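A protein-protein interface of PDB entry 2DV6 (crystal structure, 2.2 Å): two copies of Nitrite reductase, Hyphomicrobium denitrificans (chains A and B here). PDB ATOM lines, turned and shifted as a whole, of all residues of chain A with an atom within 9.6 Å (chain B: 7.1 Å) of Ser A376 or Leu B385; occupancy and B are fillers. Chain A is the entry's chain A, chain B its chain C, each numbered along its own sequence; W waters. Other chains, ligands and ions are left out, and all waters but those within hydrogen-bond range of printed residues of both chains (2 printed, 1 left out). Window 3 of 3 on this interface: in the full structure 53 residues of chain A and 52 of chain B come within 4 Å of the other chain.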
ATOM      1  N   ILE A 252       2.842   9.143  -3.218  1.00  0.00           N
ATOM      2  CA  ILE A 252       4.239   8.683  -3.238  1.00  0.00           C
ATOM      3  C   ILE A 252       4.425   7.537  -4.228  1.00  0.00           C
ATOM      4  O   ILE A 252       3.740   6.505  -4.127  1.00  0.00           O
ATOM      5  CB  ILE A 252       4.702   8.249  -1.814  1.00  0.00           C
ATOM      6  CG1 ILE A 252       4.507   9.415  -0.815  1.00  0.00           C
ATOM      7  CG2 ILE A 252       6.158   7.751  -1.815  1.00  0.00           C
ATOM      8  CD1 ILE A 252       4.788   9.034   0.649  1.00  0.00           C
ATOM      9  N   PRO A 253       5.382   7.694  -5.172  1.00  0.00           N
ATOM     10  CA  PRO A 253       5.589   6.615  -6.132  1.00  0.00           C
ATOM     11  C   PRO A 253       6.118   5.388  -5.402  1.00  0.00           C
ATOM     12  O   PRO A 253       6.756   5.531  -4.362  1.00  0.00           O
ATOM     13  CB  PRO A 253       6.662   7.167  -7.088  1.00  0.00           C
ATOM     14  CG  PRO A 253       6.848   8.579  -6.745  1.00  0.00           C
ATOM     15  CD  PRO A 253       6.353   8.793  -5.348  1.00  0.00           C
ATOM     16  N   GLY A 254       5.856   4.199  -5.940  1.00  0.00           N
ATOM     17  CA  GLY A 254       6.344   2.955  -5.351  1.00  0.00           C
ATOM     18  C   GLY A 254       5.546   1.816  -5.939  1.00  0.00           C
ATOM     19  O   GLY A 254       4.603   2.031  -6.692  1.00  0.00           O
ATOM     20  N   ILE A 255       5.950   0.597  -5.614  1.00  0.00           N
ATOM     21  CA  ILE A 255       5.229  -0.593  -5.983  1.00  0.00           C
ATOM     22  C   ILE A 255       4.632  -1.217  -4.694  1.00  0.00           C
ATOM     23  O   ILE A 255       5.374  -1.716  -3.837  1.00  0.00           O
ATOM     24  CB  ILE A 255       6.164  -1.598  -6.751  1.00  0.00           C
ATOM     25  CG1 ILE A 255       5.407  -2.851  -7.149  1.00  0.00           C
ATOM     26  CG2 ILE A 255       7.430  -1.955  -5.931  1.00  0.00           C
ATOM     27  CD1 ILE A 255       4.190  -2.604  -8.119  1.00  0.00           C
ATOM     28  N   HIS A 373      18.903  -4.756 -12.153  1.00  0.00           N
ATOM     29  CA  HIS A 373      18.434  -3.753 -11.182  1.00  0.00           C
ATOM     30  C   HIS A 373      17.415  -4.343 -10.232  1.00  0.00           C
ATOM     31  O   HIS A 373      16.476  -5.040 -10.650  1.00  0.00           O
ATOM     32  CB  HIS A 373      17.829  -2.501 -11.864  1.00  0.00           C
ATOM     33  CG  HIS A 373      18.784  -1.828 -12.801  1.00  0.00           C
ATOM     34  ND1 HIS A 373      19.804  -1.000 -12.363  1.00  0.00           N
ATOM     35  CD2 HIS A 373      18.936  -1.929 -14.145  1.00  0.00           C
ATOM     36  CE1 HIS A 373      20.501  -0.576 -13.406  1.00  0.00           C
ATOM     37  NE2 HIS A 373      20.011  -1.145 -14.495  1.00  0.00           N
ATOM     38  N   VAL A 374      17.607  -4.035  -8.947  1.00  0.00           N
ATOM     39  CA  VAL A 374      16.670  -4.422  -7.905  1.00  0.00           C
ATOM     40  C   VAL A 374      16.229  -3.163  -7.190  1.00  0.00           C
ATOM     41  O   VAL A 374      17.073  -2.390  -6.667  1.00  0.00           O
ATOM     42  CB  VAL A 374      17.333  -5.406  -6.891  1.00  0.00           C
ATOM     43  CG1 VAL A 374      16.439  -5.574  -5.665  1.00  0.00           C
ATOM     44  CG2 VAL A 374      17.610  -6.729  -7.566  1.00  0.00           C
ATOM     45  N   TYR A 375      14.917  -2.940  -7.169  1.00  0.00           N
ATOM     46  CA  TYR A 375      14.340  -1.765  -6.476  1.00  0.00           C
ATOM     47  C   TYR A 375      14.168  -2.059  -4.984  1.00  0.00           C
ATOM     48  O   TYR A 375      13.104  -2.545  -4.570  1.00  0.00           O
ATOM     49  CB  TYR A 375      13.032  -1.292  -7.168  1.00  0.00           C
ATOM     50  CG  TYR A 375      13.333  -0.633  -8.519  1.00  0.00           C
ATOM     51  CD1 TYR A 375      13.605  -1.410  -9.655  1.00  0.00           C
ATOM     52  CD2 TYR A 375      13.418   0.742  -8.644  1.00  0.00           C
ATOM     53  CE1 TYR A 375      13.915  -0.834 -10.880  1.00  0.00           C
ATOM     54  CE2 TYR A 375      13.753   1.351  -9.882  1.00  0.00           C
ATOM     55  CZ  TYR A 375      13.980   0.553 -11.005  1.00  0.00           C
ATOM     56  OH  TYR A 375      14.297   1.120 -12.244  1.00  0.00           O
ATOM     57  N   SER A 376      15.220  -1.813  -4.181  1.00  0.00           N
ATOM     58  CA  SER A 376      15.208  -2.249  -2.761  1.00  0.00           C
ATOM     59  C   SER A 376      13.938  -1.824  -2.029  1.00  0.00           C
ATOM     60  O   SER A 376      13.596  -0.656  -2.065  1.00  0.00           O
ATOM     61  CB  SER A 376      16.380  -1.690  -1.940  1.00  0.00           C
ATOM     62  OG  SER A 376      17.429  -1.196  -2.733  1.00  0.00           O
ATOM     63  N   LEU A 377      13.277  -2.765  -1.354  1.00  0.00           N
ATOM     64  CA  LEU A 377      12.108  -2.505  -0.488  1.00  0.00           C
ATOM     65  C   LEU A 377      10.931  -1.879  -1.230  1.00  0.00           C
ATOM     66  O   LEU A 377       9.994  -1.347  -0.612  1.00  0.00           O
ATOM     67  CB  LEU A 377      12.483  -1.688   0.771  1.00  0.00           C
ATOM     68  CG  LEU A 377      13.441  -2.404   1.738  1.00  0.00           C
ATOM     69  CD1 LEU A 377      13.666  -1.593   3.020  1.00  0.00           C
ATOM     70  CD2 LEU A 377      12.935  -3.831   2.068  1.00  0.00           C
ATOM     71  N   GLY A 378      10.991  -1.958  -2.555  1.00  0.00           N
ATOM     72  CA  GLY A 378       9.935  -1.438  -3.425  1.00  0.00           C
ATOM     73  C   GLY A 378      10.111   0.055  -3.691  1.00  0.00           C
ATOM     74  O   GLY A 378       9.238   0.678  -4.268  1.00  0.00           O
ATOM     75  N   SER A 379      11.230   0.629  -3.252  1.00  0.00           N
ATOM     76  CA  SER A 379      11.510   2.038  -3.513  1.00  0.00           C
ATOM     77  C   SER A 379      11.753   2.269  -4.989  1.00  0.00           C
ATOM     78  O   SER A 379      12.620   1.633  -5.629  1.00  0.00           O
ATOM     79  CB  SER A 379      12.718   2.546  -2.775  1.00  0.00           C
ATOM     80  OG  SER A 379      12.921   3.905  -3.165  1.00  0.00           O
ATOM     81  N   VAL A 380      10.981   3.207  -5.502  1.00  0.00           N
ATOM     82  CA  VAL A 380      10.995   3.582  -6.908  1.00  0.00           C
ATOM     83  C   VAL A 380      11.729   4.948  -7.061  1.00  0.00           C
ATOM     84  O   VAL A 380      12.136   5.339  -8.147  1.00  0.00           O
ATOM     85  CB  VAL A 380       9.530   3.545  -7.402  1.00  0.00           C
ATOM     86  CG1 VAL A 380       9.173   4.716  -8.210  1.00  0.00           C
ATOM     87  CG2 VAL A 380       9.165   2.154  -7.998  1.00  0.00           C
ATOM     88  N   VAL A 381      11.981   5.613  -5.940  1.00  0.00           N
ATOM     89  CA  VAL A 381      12.718   6.896  -5.912  1.00  0.00           C
ATOM     90  C   VAL A 381      14.230   6.729  -5.724  1.00  0.00           C
ATOM     91  O   VAL A 381      15.015   7.436  -6.340  1.00  0.00           O
ATOM     92  CB  VAL A 381      12.135   7.813  -4.847  1.00  0.00           C
ATOM     93  CG1 VAL A 381      12.881   9.192  -4.817  1.00  0.00           C
ATOM     94  CG2 VAL A 381      10.645   8.011  -5.109  1.00  0.00           C
ATOM     95  N   SER A 382      14.656   5.784  -4.892  1.00  0.00           N
ATOM     96  CA  SER A 382      16.091   5.558  -4.692  1.00  0.00           C
ATOM     97  C   SER A 382      16.673   4.812  -5.900  1.00  0.00           C
ATOM     98  O   SER A 382      15.940   4.097  -6.603  1.00  0.00           O
ATOM     99  CB  SER A 382      16.343   4.741  -3.416  1.00  0.00           C
ATOM    100  OG  SER A 382      15.773   5.380  -2.293  1.00  0.00           O
ATOM    101  N   PRO A 383      17.986   5.001  -6.168  1.00  0.00           N
ATOM    102  CA  PRO A 383      18.587   4.268  -7.298  1.00  0.00           C
ATOM    103  C   PRO A 383      18.563   2.761  -6.998  1.00  0.00           C
ATOM    104  O   PRO A 383      18.960   2.365  -5.911  1.00  0.00           O
ATOM    105  CB  PRO A 383      20.039   4.773  -7.342  1.00  0.00           C
ATOM    106  CG  PRO A 383      20.071   6.047  -6.457  1.00  0.00           C
ATOM    107  CD  PRO A 383      18.955   5.862  -5.447  1.00  0.00           C
ATOM    108  N   PRO A 384      18.081   1.933  -7.944  1.00  0.00           N
ATOM    109  CA  PRO A 384      18.062   0.512  -7.684  1.00  0.00           C
ATOM    110  C   PRO A 384      19.479  -0.027  -7.429  1.00  0.00           C
ATOM    111  O   PRO A 384      20.488   0.606  -7.820  1.00  0.00           O
ATOM    112  CB  PRO A 384      17.462  -0.070  -8.971  1.00  0.00           C
ATOM    113  CG  PRO A 384      17.687   0.964 -10.030  1.00  0.00           C
ATOM    114  CD  PRO A 384      17.529   2.257  -9.275  1.00  0.00           C
ATOM    115  N   LEU A 385      19.552  -1.169  -6.739  1.00  0.00           N
ATOM    116  CA  LEU A 385      20.810  -1.908  -6.590  1.00  0.00           C
ATOM    117  C   LEU A 385      21.155  -2.604  -7.900  1.00  0.00           C
ATOM    118  O   LEU A 385      20.259  -2.970  -8.679  1.00  0.00           O
ATOM    119  CB  LEU A 385      20.684  -2.964  -5.473  1.00  0.00           C
ATOM    120  CG  LEU A 385      20.492  -2.451  -4.052  1.00  0.00           C
ATOM    121  CD1 LEU A 385      20.416  -3.635  -3.063  1.00  0.00           C
ATOM    122  CD2 LEU A 385      21.654  -1.516  -3.686  1.00  0.00           C
ATOM    123  N   ILE A 386      22.447  -2.838  -8.120  1.00  0.00           N
ATOM    124  CA  ILE A 386      22.931  -3.404  -9.399  1.00  0.00           C
ATOM    125  C   ILE A 386      23.549  -4.794  -9.256  1.00  0.00           C
ATOM    126  O   ILE A 386      24.406  -5.001  -8.432  1.00  0.00           O
ATOM    127  CB  ILE A 386      23.949  -2.432 -10.096  1.00  0.00           C
ATOM    128  CG1 ILE A 386      23.310  -1.053 -10.319  1.00  0.00           C
ATOM    129  CG2 ILE A 386      24.486  -3.011 -11.437  1.00  0.00           C
ATOM    130  CD1 ILE A 386      24.292   0.107 -10.164  1.00  0.00           C
ATOM    131  N   VAL A 388      22.377  -8.334  -8.843  1.00  0.00           N
ATOM    132  CA  VAL A 388      21.963  -9.022  -7.614  1.00  0.00           C
ATOM    133  C   VAL A 388      21.356 -10.390  -7.946  1.00  0.00           C
ATOM    134  O   VAL A 388      20.531 -10.492  -8.872  1.00  0.00           O
ATOM    135  CB  VAL A 388      20.931  -8.152  -6.833  1.00  0.00           C
ATOM    136  CG1 VAL A 388      20.291  -8.955  -5.643  1.00  0.00           C
ATOM    137  CG2 VAL A 388      21.565  -6.864  -6.350  1.00  0.00           C
ATOM    138  N   VAL A 391      16.715 -11.576  -3.975  1.00  0.00           N
ATOM    139  CA  VAL A 391      16.176 -10.441  -3.200  1.00  0.00           C
ATOM    140  C   VAL A 391      15.200 -10.935  -2.121  1.00  0.00           C
ATOM    141  O   VAL A 391      14.330 -11.753  -2.455  1.00  0.00           O
ATOM    142  CB  VAL A 391      15.550  -9.343  -4.150  1.00  0.00           C
ATOM    143  CG1 VAL A 391      14.528  -9.923  -5.057  1.00  0.00           C
ATOM    144  CG2 VAL A 391      14.977  -8.133  -3.346  1.00  0.00           C
ATOM    145  N   SER A 392      15.377 -10.507  -0.855  1.00  0.00           N
ATOM    146  CA  SER A 392      14.384 -10.792   0.212  1.00  0.00           C
ATOM    147  C   SER A 392      13.240  -9.820   0.095  1.00  0.00           C
ATOM    148  O   SER A 392      13.478  -8.599   0.041  1.00  0.00           O
ATOM    149  CB  SER A 392      14.903 -10.618   1.653  1.00  0.00           C
ATOM    150  OG  SER A 392      15.945 -11.488   1.925  1.00  0.00           O
ATOM    151  N   VAL A 393      12.026 -10.366   0.076  1.00  0.00           N
ATOM    152  CA  VAL A 393      10.805  -9.599  -0.088  1.00  0.00           C
ATOM    153  C   VAL A 393       9.869 -10.012   1.058  1.00  0.00           C
ATOM    154  O   VAL A 393       9.409 -11.151   1.108  1.00  0.00           O
ATOM    155  CB  VAL A 393      10.109  -9.878  -1.431  1.00  0.00           C
ATOM    156  CG1 VAL A 393       8.859  -8.983  -1.553  1.00  0.00           C
ATOM    157  CG2 VAL A 393      11.059  -9.606  -2.594  1.00  0.00           C
ATOM    158  N   PRO A 394       9.613  -9.094   1.993  1.00  0.00           N
ATOM    159  CA  PRO A 394       8.814  -9.494   3.139  1.00  0.00           C
ATOM    160  C   PRO A 394       7.324  -9.597   2.756  1.00  0.00           C
ATOM    161  O   PRO A 394       6.909  -9.026   1.742  1.00  0.00           O
ATOM    162  CB  PRO A 394       9.026  -8.346   4.120  1.00  0.00           C
ATOM    163  CG  PRO A 394       9.183  -7.120   3.198  1.00  0.00           C
ATOM    164  CD  PRO A 394      10.041  -7.682   2.063  1.00  0.00           C
ATOM    165  N   GLY A 397       5.183  -6.672   1.250  1.00  0.00           N
ATOM    166  CA  GLY A 397       6.188  -5.901   0.546  1.00  0.00           C
ATOM    167  C   GLY A 397       6.250  -6.353  -0.913  1.00  0.00           C
ATOM    168  O   GLY A 397       5.758  -7.429  -1.261  1.00  0.00           O
ATOM    169  N   ALA A 398       6.826  -5.502  -1.765  1.00  0.00           N
ATOM    170  CA  ALA A 398       6.972  -5.792  -3.198  1.00  0.00           C
ATOM    171  C   ALA A 398       8.305  -5.225  -3.676  1.00  0.00           C
ATOM    172  O   ALA A 398       8.882  -4.367  -3.002  1.00  0.00           O
ATOM    173  CB  ALA A 398       5.827  -5.208  -3.969  1.00  0.00           C
ATOM    174  N   THR A 399       8.815  -5.741  -4.793  1.00  0.00           N
ATOM    175  CA  THR A 399       9.949  -5.106  -5.500  1.00  0.00           C
ATOM    176  C   THR A 399       9.740  -5.143  -6.998  1.00  0.00           C
ATOM    177  O   THR A 399       8.829  -5.753  -7.505  1.00  0.00           O
ATOM    178  CB  THR A 399      11.215  -5.836  -5.043  1.00  0.00           C
ATOM    179  OG1 THR A 399      12.528  -5.277  -5.328  1.00  0.00           O
ATOM    180  CG2 THR A 399      11.155  -7.350  -5.235  1.00  0.00           C
ATOM    181  N   ILE A 400      10.711  -4.568  -7.677  1.00  0.00           N
ATOM    182  CA  ILE A 400      10.809  -4.560  -9.109  1.00  0.00           C
ATOM    183  C   ILE A 400      12.201  -5.093  -9.417  1.00  0.00           C
ATOM    184  O   ILE A 400      13.198  -4.663  -8.804  1.00  0.00           O
ATOM    185  CB  ILE A 400      10.653  -3.117  -9.640  1.00  0.00           C
ATOM    186  CG1 ILE A 400       9.223  -2.626  -9.398  1.00  0.00           C
ATOM    187  CG2 ILE A 400      10.984  -3.057 -11.161  1.00  0.00           C
ATOM    188  CD1 ILE A 400       9.020  -1.109  -9.614  1.00  0.00           C
ATOM    189  N   VAL A 401      12.266  -6.079 -10.301  1.00  0.00           N
ATOM    190  CA  VAL A 401      13.567  -6.537 -10.815  1.00  0.00           C
ATOM    191  C   VAL A 401      13.540  -6.394 -12.333  1.00  0.00           C
ATOM    192  O   VAL A 401      12.493  -6.654 -12.955  1.00  0.00           O
ATOM    193  CB  VAL A 401      13.929  -7.974 -10.336  1.00  0.00           C
ATOM    194  CG1 VAL A 401      14.012  -8.028  -8.772  1.00  0.00           C
ATOM    195  CG2 VAL A 401      12.949  -9.007 -10.868  1.00  0.00           C
ATOM    196  N   PHE B 371       6.599   4.966   4.550  1.00  0.00           N
ATOM    197  CA  PHE B 371       7.814   5.540   5.123  1.00  0.00           C
ATOM    198  C   PHE B 371       8.475   6.474   4.082  1.00  0.00           C
ATOM    199  O   PHE B 371       8.807   6.044   2.956  1.00  0.00           O
ATOM    200  CB  PHE B 371       8.792   4.459   5.594  1.00  0.00           C
ATOM    201  CG  PHE B 371       8.195   3.468   6.582  1.00  0.00           C
ATOM    202  CD1 PHE B 371       8.289   2.091   6.344  1.00  0.00           C
ATOM    203  CD2 PHE B 371       7.529   3.897   7.732  1.00  0.00           C
ATOM    204  CE1 PHE B 371       7.763   1.174   7.230  1.00  0.00           C
ATOM    205  CE2 PHE B 371       6.980   2.970   8.637  1.00  0.00           C
ATOM    206  CZ  PHE B 371       7.105   1.594   8.382  1.00  0.00           C
ATOM    207  N   ASP B 372       8.637   7.741   4.445  1.00  0.00           N
ATOM    208  CA  ASP B 372       9.312   8.719   3.583  1.00  0.00           C
ATOM    209  C   ASP B 372      10.789   8.366   3.463  1.00  0.00           C
ATOM    210  O   ASP B 372      11.328   8.404   2.361  1.00  0.00           O
ATOM    211  CB  ASP B 372       9.160  10.149   4.136  1.00  0.00           C
ATOM    212  CG  ASP B 372       7.758  10.695   3.945  1.00  0.00           C
ATOM    213  OD1 ASP B 372       7.048  10.257   3.017  1.00  0.00           O
ATOM    214  OD2 ASP B 372       7.335  11.541   4.751  1.00  0.00           O
ATOM    215  N   HIS B 373      11.417   8.049   4.605  1.00  0.00           N
ATOM    216  CA  HIS B 373      12.806   7.583   4.696  1.00  0.00           C
ATOM    217  C   HIS B 373      12.950   6.316   5.527  1.00  0.00           C
ATOM    218  O   HIS B 373      12.309   6.173   6.576  1.00  0.00           O
ATOM    219  CB  HIS B 373      13.731   8.689   5.239  1.00  0.00           C
ATOM    220  CG  HIS B 373      13.773   9.882   4.349  1.00  0.00           C
ATOM    221  ND1 HIS B 373      12.932  10.961   4.517  1.00  0.00           N
ATOM    222  CD2 HIS B 373      14.482  10.127   3.217  1.00  0.00           C
ATOM    223  CE1 HIS B 373      13.145  11.834   3.542  1.00  0.00           C
ATOM    224  NE2 HIS B 373      14.094  11.358   2.754  1.00  0.00           N
ATOM    225  N   VAL B 374      13.756   5.377   5.007  1.00  0.00           N
ATOM    226  CA  VAL B 374      14.139   4.170   5.713  1.00  0.00           C
ATOM    227  C   VAL B 374      15.659   4.081   5.751  1.00  0.00           C
ATOM    228  O   VAL B 374      16.298   4.016   4.721  1.00  0.00           O
ATOM    229  CB  VAL B 374      13.577   2.909   5.051  1.00  0.00           C
ATOM    230  CG1 VAL B 374      14.052   1.632   5.789  1.00  0.00           C
ATOM    231  CG2 VAL B 374      12.062   2.968   4.991  1.00  0.00           C
ATOM    232  N   TYR B 375      16.212   4.055   6.960  1.00  0.00           N
ATOM    233  CA  TYR B 375      17.639   3.881   7.184  1.00  0.00           C
ATOM    234  C   TYR B 375      17.998   2.400   7.110  1.00  0.00           C
ATOM    235  O   TYR B 375      17.936   1.689   8.130  1.00  0.00           O
ATOM    236  CB  TYR B 375      18.010   4.501   8.544  1.00  0.00           C
ATOM    237  CG  TYR B 375      17.925   6.019   8.499  1.00  0.00           C
ATOM    238  CD1 TYR B 375      16.679   6.669   8.512  1.00  0.00           C
ATOM    239  CD2 TYR B 375      19.090   6.801   8.407  1.00  0.00           C
ATOM    240  CE1 TYR B 375      16.583   8.074   8.449  1.00  0.00           C
ATOM    241  CE2 TYR B 375      19.034   8.215   8.351  1.00  0.00           C
ATOM    242  CZ  TYR B 375      17.773   8.838   8.374  1.00  0.00           C
ATOM    243  OH  TYR B 375      17.703  10.198   8.301  1.00  0.00           O
ATOM    244  N   SER B 376      18.352   1.933   5.902  1.00  0.00           N
ATOM    245  CA  SER B 376      18.494   0.486   5.661  1.00  0.00           C
ATOM    246  C   SER B 376      19.523  -0.125   6.590  1.00  0.00           C
ATOM    247  O   SER B 376      20.626   0.409   6.742  1.00  0.00           O
ATOM    248  CB  SER B 376      18.888   0.106   4.194  1.00  0.00           C
ATOM    249  OG  SER B 376      18.987   1.220   3.332  1.00  0.00           O
ATOM    250  N   SER B 382      24.824   6.044   5.536  1.00  0.00           N
ATOM    251  CA  SER B 382      24.397   5.854   4.135  1.00  0.00           C
ATOM    252  C   SER B 382      23.086   6.594   3.934  1.00  0.00           C
ATOM    253  O   SER B 382      22.341   6.781   4.914  1.00  0.00           O
ATOM    254  CB  SER B 382      24.200   4.379   3.839  1.00  0.00           C
ATOM    255  OG  SER B 382      25.447   3.726   3.736  1.00  0.00           O
ATOM    256  N   PRO B 383      22.811   7.056   2.690  1.00  0.00           N
ATOM    257  CA  PRO B 383      21.539   7.720   2.383  1.00  0.00           C
ATOM    258  C   PRO B 383      20.358   6.782   2.605  1.00  0.00           C
ATOM    259  O   PRO B 383      20.352   5.648   2.087  1.00  0.00           O
ATOM    260  CB  PRO B 383      21.647   8.057   0.879  1.00  0.00           C
ATOM    261  CG  PRO B 383      23.147   8.116   0.605  1.00  0.00           C
ATOM    262  CD  PRO B 383      23.701   7.004   1.512  1.00  0.00           C
ATOM    263  N   PRO B 384      19.351   7.259   3.345  1.00  0.00           N
ATOM    264  CA  PRO B 384      18.130   6.490   3.600  1.00  0.00           C
ATOM    265  C   PRO B 384      17.444   6.176   2.254  1.00  0.00           C
ATOM    266  O   PRO B 384      17.613   6.946   1.283  1.00  0.00           O
ATOM    267  CB  PRO B 384      17.263   7.463   4.408  1.00  0.00           C
ATOM    268  CG  PRO B 384      18.183   8.508   4.879  1.00  0.00           C
ATOM    269  CD  PRO B 384      19.335   8.591   3.967  1.00  0.00           C
ATOM    270  N   LEU B 385      16.705   5.070   2.196  1.00  0.00           N
ATOM    271  CA  LEU B 385      15.801   4.776   1.061  1.00  0.00           C
ATOM    272  C   LEU B 385      14.527   5.600   1.154  1.00  0.00           C
ATOM    273  O   LEU B 385      14.079   5.941   2.244  1.00  0.00           O
ATOM    274  CB  LEU B 385      15.422   3.299   1.018  1.00  0.00           C
ATOM    275  CG  LEU B 385      16.553   2.301   0.794  1.00  0.00           C
ATOM    276  CD1 LEU B 385      16.063   0.864   1.046  1.00  0.00           C
ATOM    277  CD2 LEU B 385      17.107   2.494  -0.630  1.00  0.00           C
ATOM    278  N   ILE B 386      13.940   5.908   0.006  1.00  0.00           N
ATOM    279  CA  ILE B 386      12.823   6.854  -0.050  1.00  0.00           C
ATOM    280  C   ILE B 386      11.552   6.163  -0.495  1.00  0.00           C
ATOM    281  O   ILE B 386      11.556   5.453  -1.506  1.00  0.00           O
ATOM    282  CB  ILE B 386      13.142   8.080  -1.029  1.00  0.00           C
ATOM    283  CG1 ILE B 386      14.377   8.827  -0.559  1.00  0.00           C
ATOM    284  CG2 ILE B 386      11.949   9.051  -1.155  1.00  0.00           C
ATOM    285  CD1 ILE B 386      15.100   9.618  -1.676  1.00  0.00           C
ATOM    286  N   GLY B 387      10.464   6.367   0.249  1.00  0.00           N
ATOM    287  CA  GLY B 387       9.154   5.929  -0.221  1.00  0.00           C
ATOM    288  C   GLY B 387       8.989   4.414  -0.160  1.00  0.00           C
ATOM    289  O   GLY B 387       8.945   3.737  -1.204  1.00  0.00           O
ATOM    290  N   VAL B 388       8.847   3.894   1.064  1.00  0.00           N
ATOM    291  CA  VAL B 388       8.907   2.446   1.320  1.00  0.00           C
ATOM    292  C   VAL B 388       7.713   1.984   2.168  1.00  0.00           C
ATOM    293  O   VAL B 388       7.411   2.592   3.183  1.00  0.00           O
ATOM    294  CB  VAL B 388      10.253   2.083   1.993  1.00  0.00           C
ATOM    295  CG1 VAL B 388      10.219   0.660   2.602  1.00  0.00           C
ATOM    296  CG2 VAL B 388      11.410   2.219   0.977  1.00  0.00           C
HETATM  297  O   HOH W   1      18.041   6.585  -1.306  1.00  0.00           O
HETATM  298  O   HOH W   2       7.394   1.667  -2.522  1.00  0.00           O
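OG of Ser A379 lies within hydrogen-bond range of O of Ile B386. OG of Ser A382 lies within hydrogen-bond range of N of Ile B386 (3.0 Å).
The side-chain hydroxyl (OG) of Ser A379 is in hydrogen-bond range of the backbone NH (N) of Val A381 (3.4 Å). OG of Ser A379 lies within hydrogen-bond range of N of Ser A382, 3.1 Å away. O of Phe B371 is in hydrogen-bond range of N of Gly B387, 3.2 Å away. The backbone carbonyl oxygen of Val B388 is in hydrogen-bond range of the backbone NH of Phe B371 (2.9 Å). N of Gly B387 is in hydrogen-bond range of O of Asp B372, at 3.1 Å. The backbone NH (N) of Leu B385 lies within hydrogen-bond range of the backbone carbonyl oxygen (O) of Val B374 (2.8 Å).
Among the printed residues, pairs that only touch across the chains: Ile A252 with Asp B372 (3.5 Å), Ile A252 with Gly B387 (3.9 Å), Ser A376 with Leu B385 (3.9 Å), Leu A377 with Leu B385 (3.96 Å), Leu A377 with Val B388 (3.7 Å), Ser A379 with Gly B387 (3.8 Å), Ser A379 with Val B388 (3.99 Å), Val A381 with Ile B386 (3.8 Å) and Ser A382 with Leu B385 (3.4 Å).
Printed residues of chain B within 4 Å of Ser A376: Leu B385. No residue of chain A comes within 4 Å of Val B374. No residue of chain A comes within 4 Å of Pro B384. Printed residues of chain B within 4 Å of Ile A252: Asp B372 and Gly B387. Of the printed residues of chain A, Gly B387 touches Ile A252 (3.9 Å) and Ser A379 (3.8 Å). Printed residues of chain B within 4 Å of Ser A382: Leu B385 (3.4 Å) and Ile B386 (3.0 Å). Of the printed residues of chain B, Ser A379 touches Ile B386, Gly B387 and Val B388. Of the printed residues of chain B, Val A381 touches Ile B386. Val A388 touches none of the printed residues of chain B. The nearest residue of chain A that does not touch Leu B385 is Ser A379 (4.7 Å).
Hydrophobic or aromatic side chains of chain A that line the printed part of chain B: Ile A252, Leu A377 and Val A381. Hydrophobic or aromatic side chains of chain B within 4 Å of the printed part of chain A: Leu B385, Ile B386 and Val B388. Among the printed residues, 11 pairs touch across the chains. Among the printed residues, no Asp or Glu carboxylate lies within 4 Å of a Lys or Arg side-chain nitrogen of the other chain.
Ser A376 touches Leu B385, but with the chains exchanged Leu A385 does not touch Ser B376 (8.0 Å). Ser A382 touches Leu B385, but with the chains exchanged Leu A385 does not touch Ser B382 (9.8 Å). Ser A382 touches Ile B386, but with the chains exchanged Ile A386 does not touch Ser B382 (13.9 Å). Of the 11 pairs that touch across the chains among the printed residues, none has its exchanged pair printed and touching as well.
Water W1 lies within hydrogen-bond range of O of Pro B384 and OG of Ser A382. Water W2 lies within hydrogen-bond range of O of Gly A378 (2.7 Å) and O of Gly B387 (2.9 Å).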
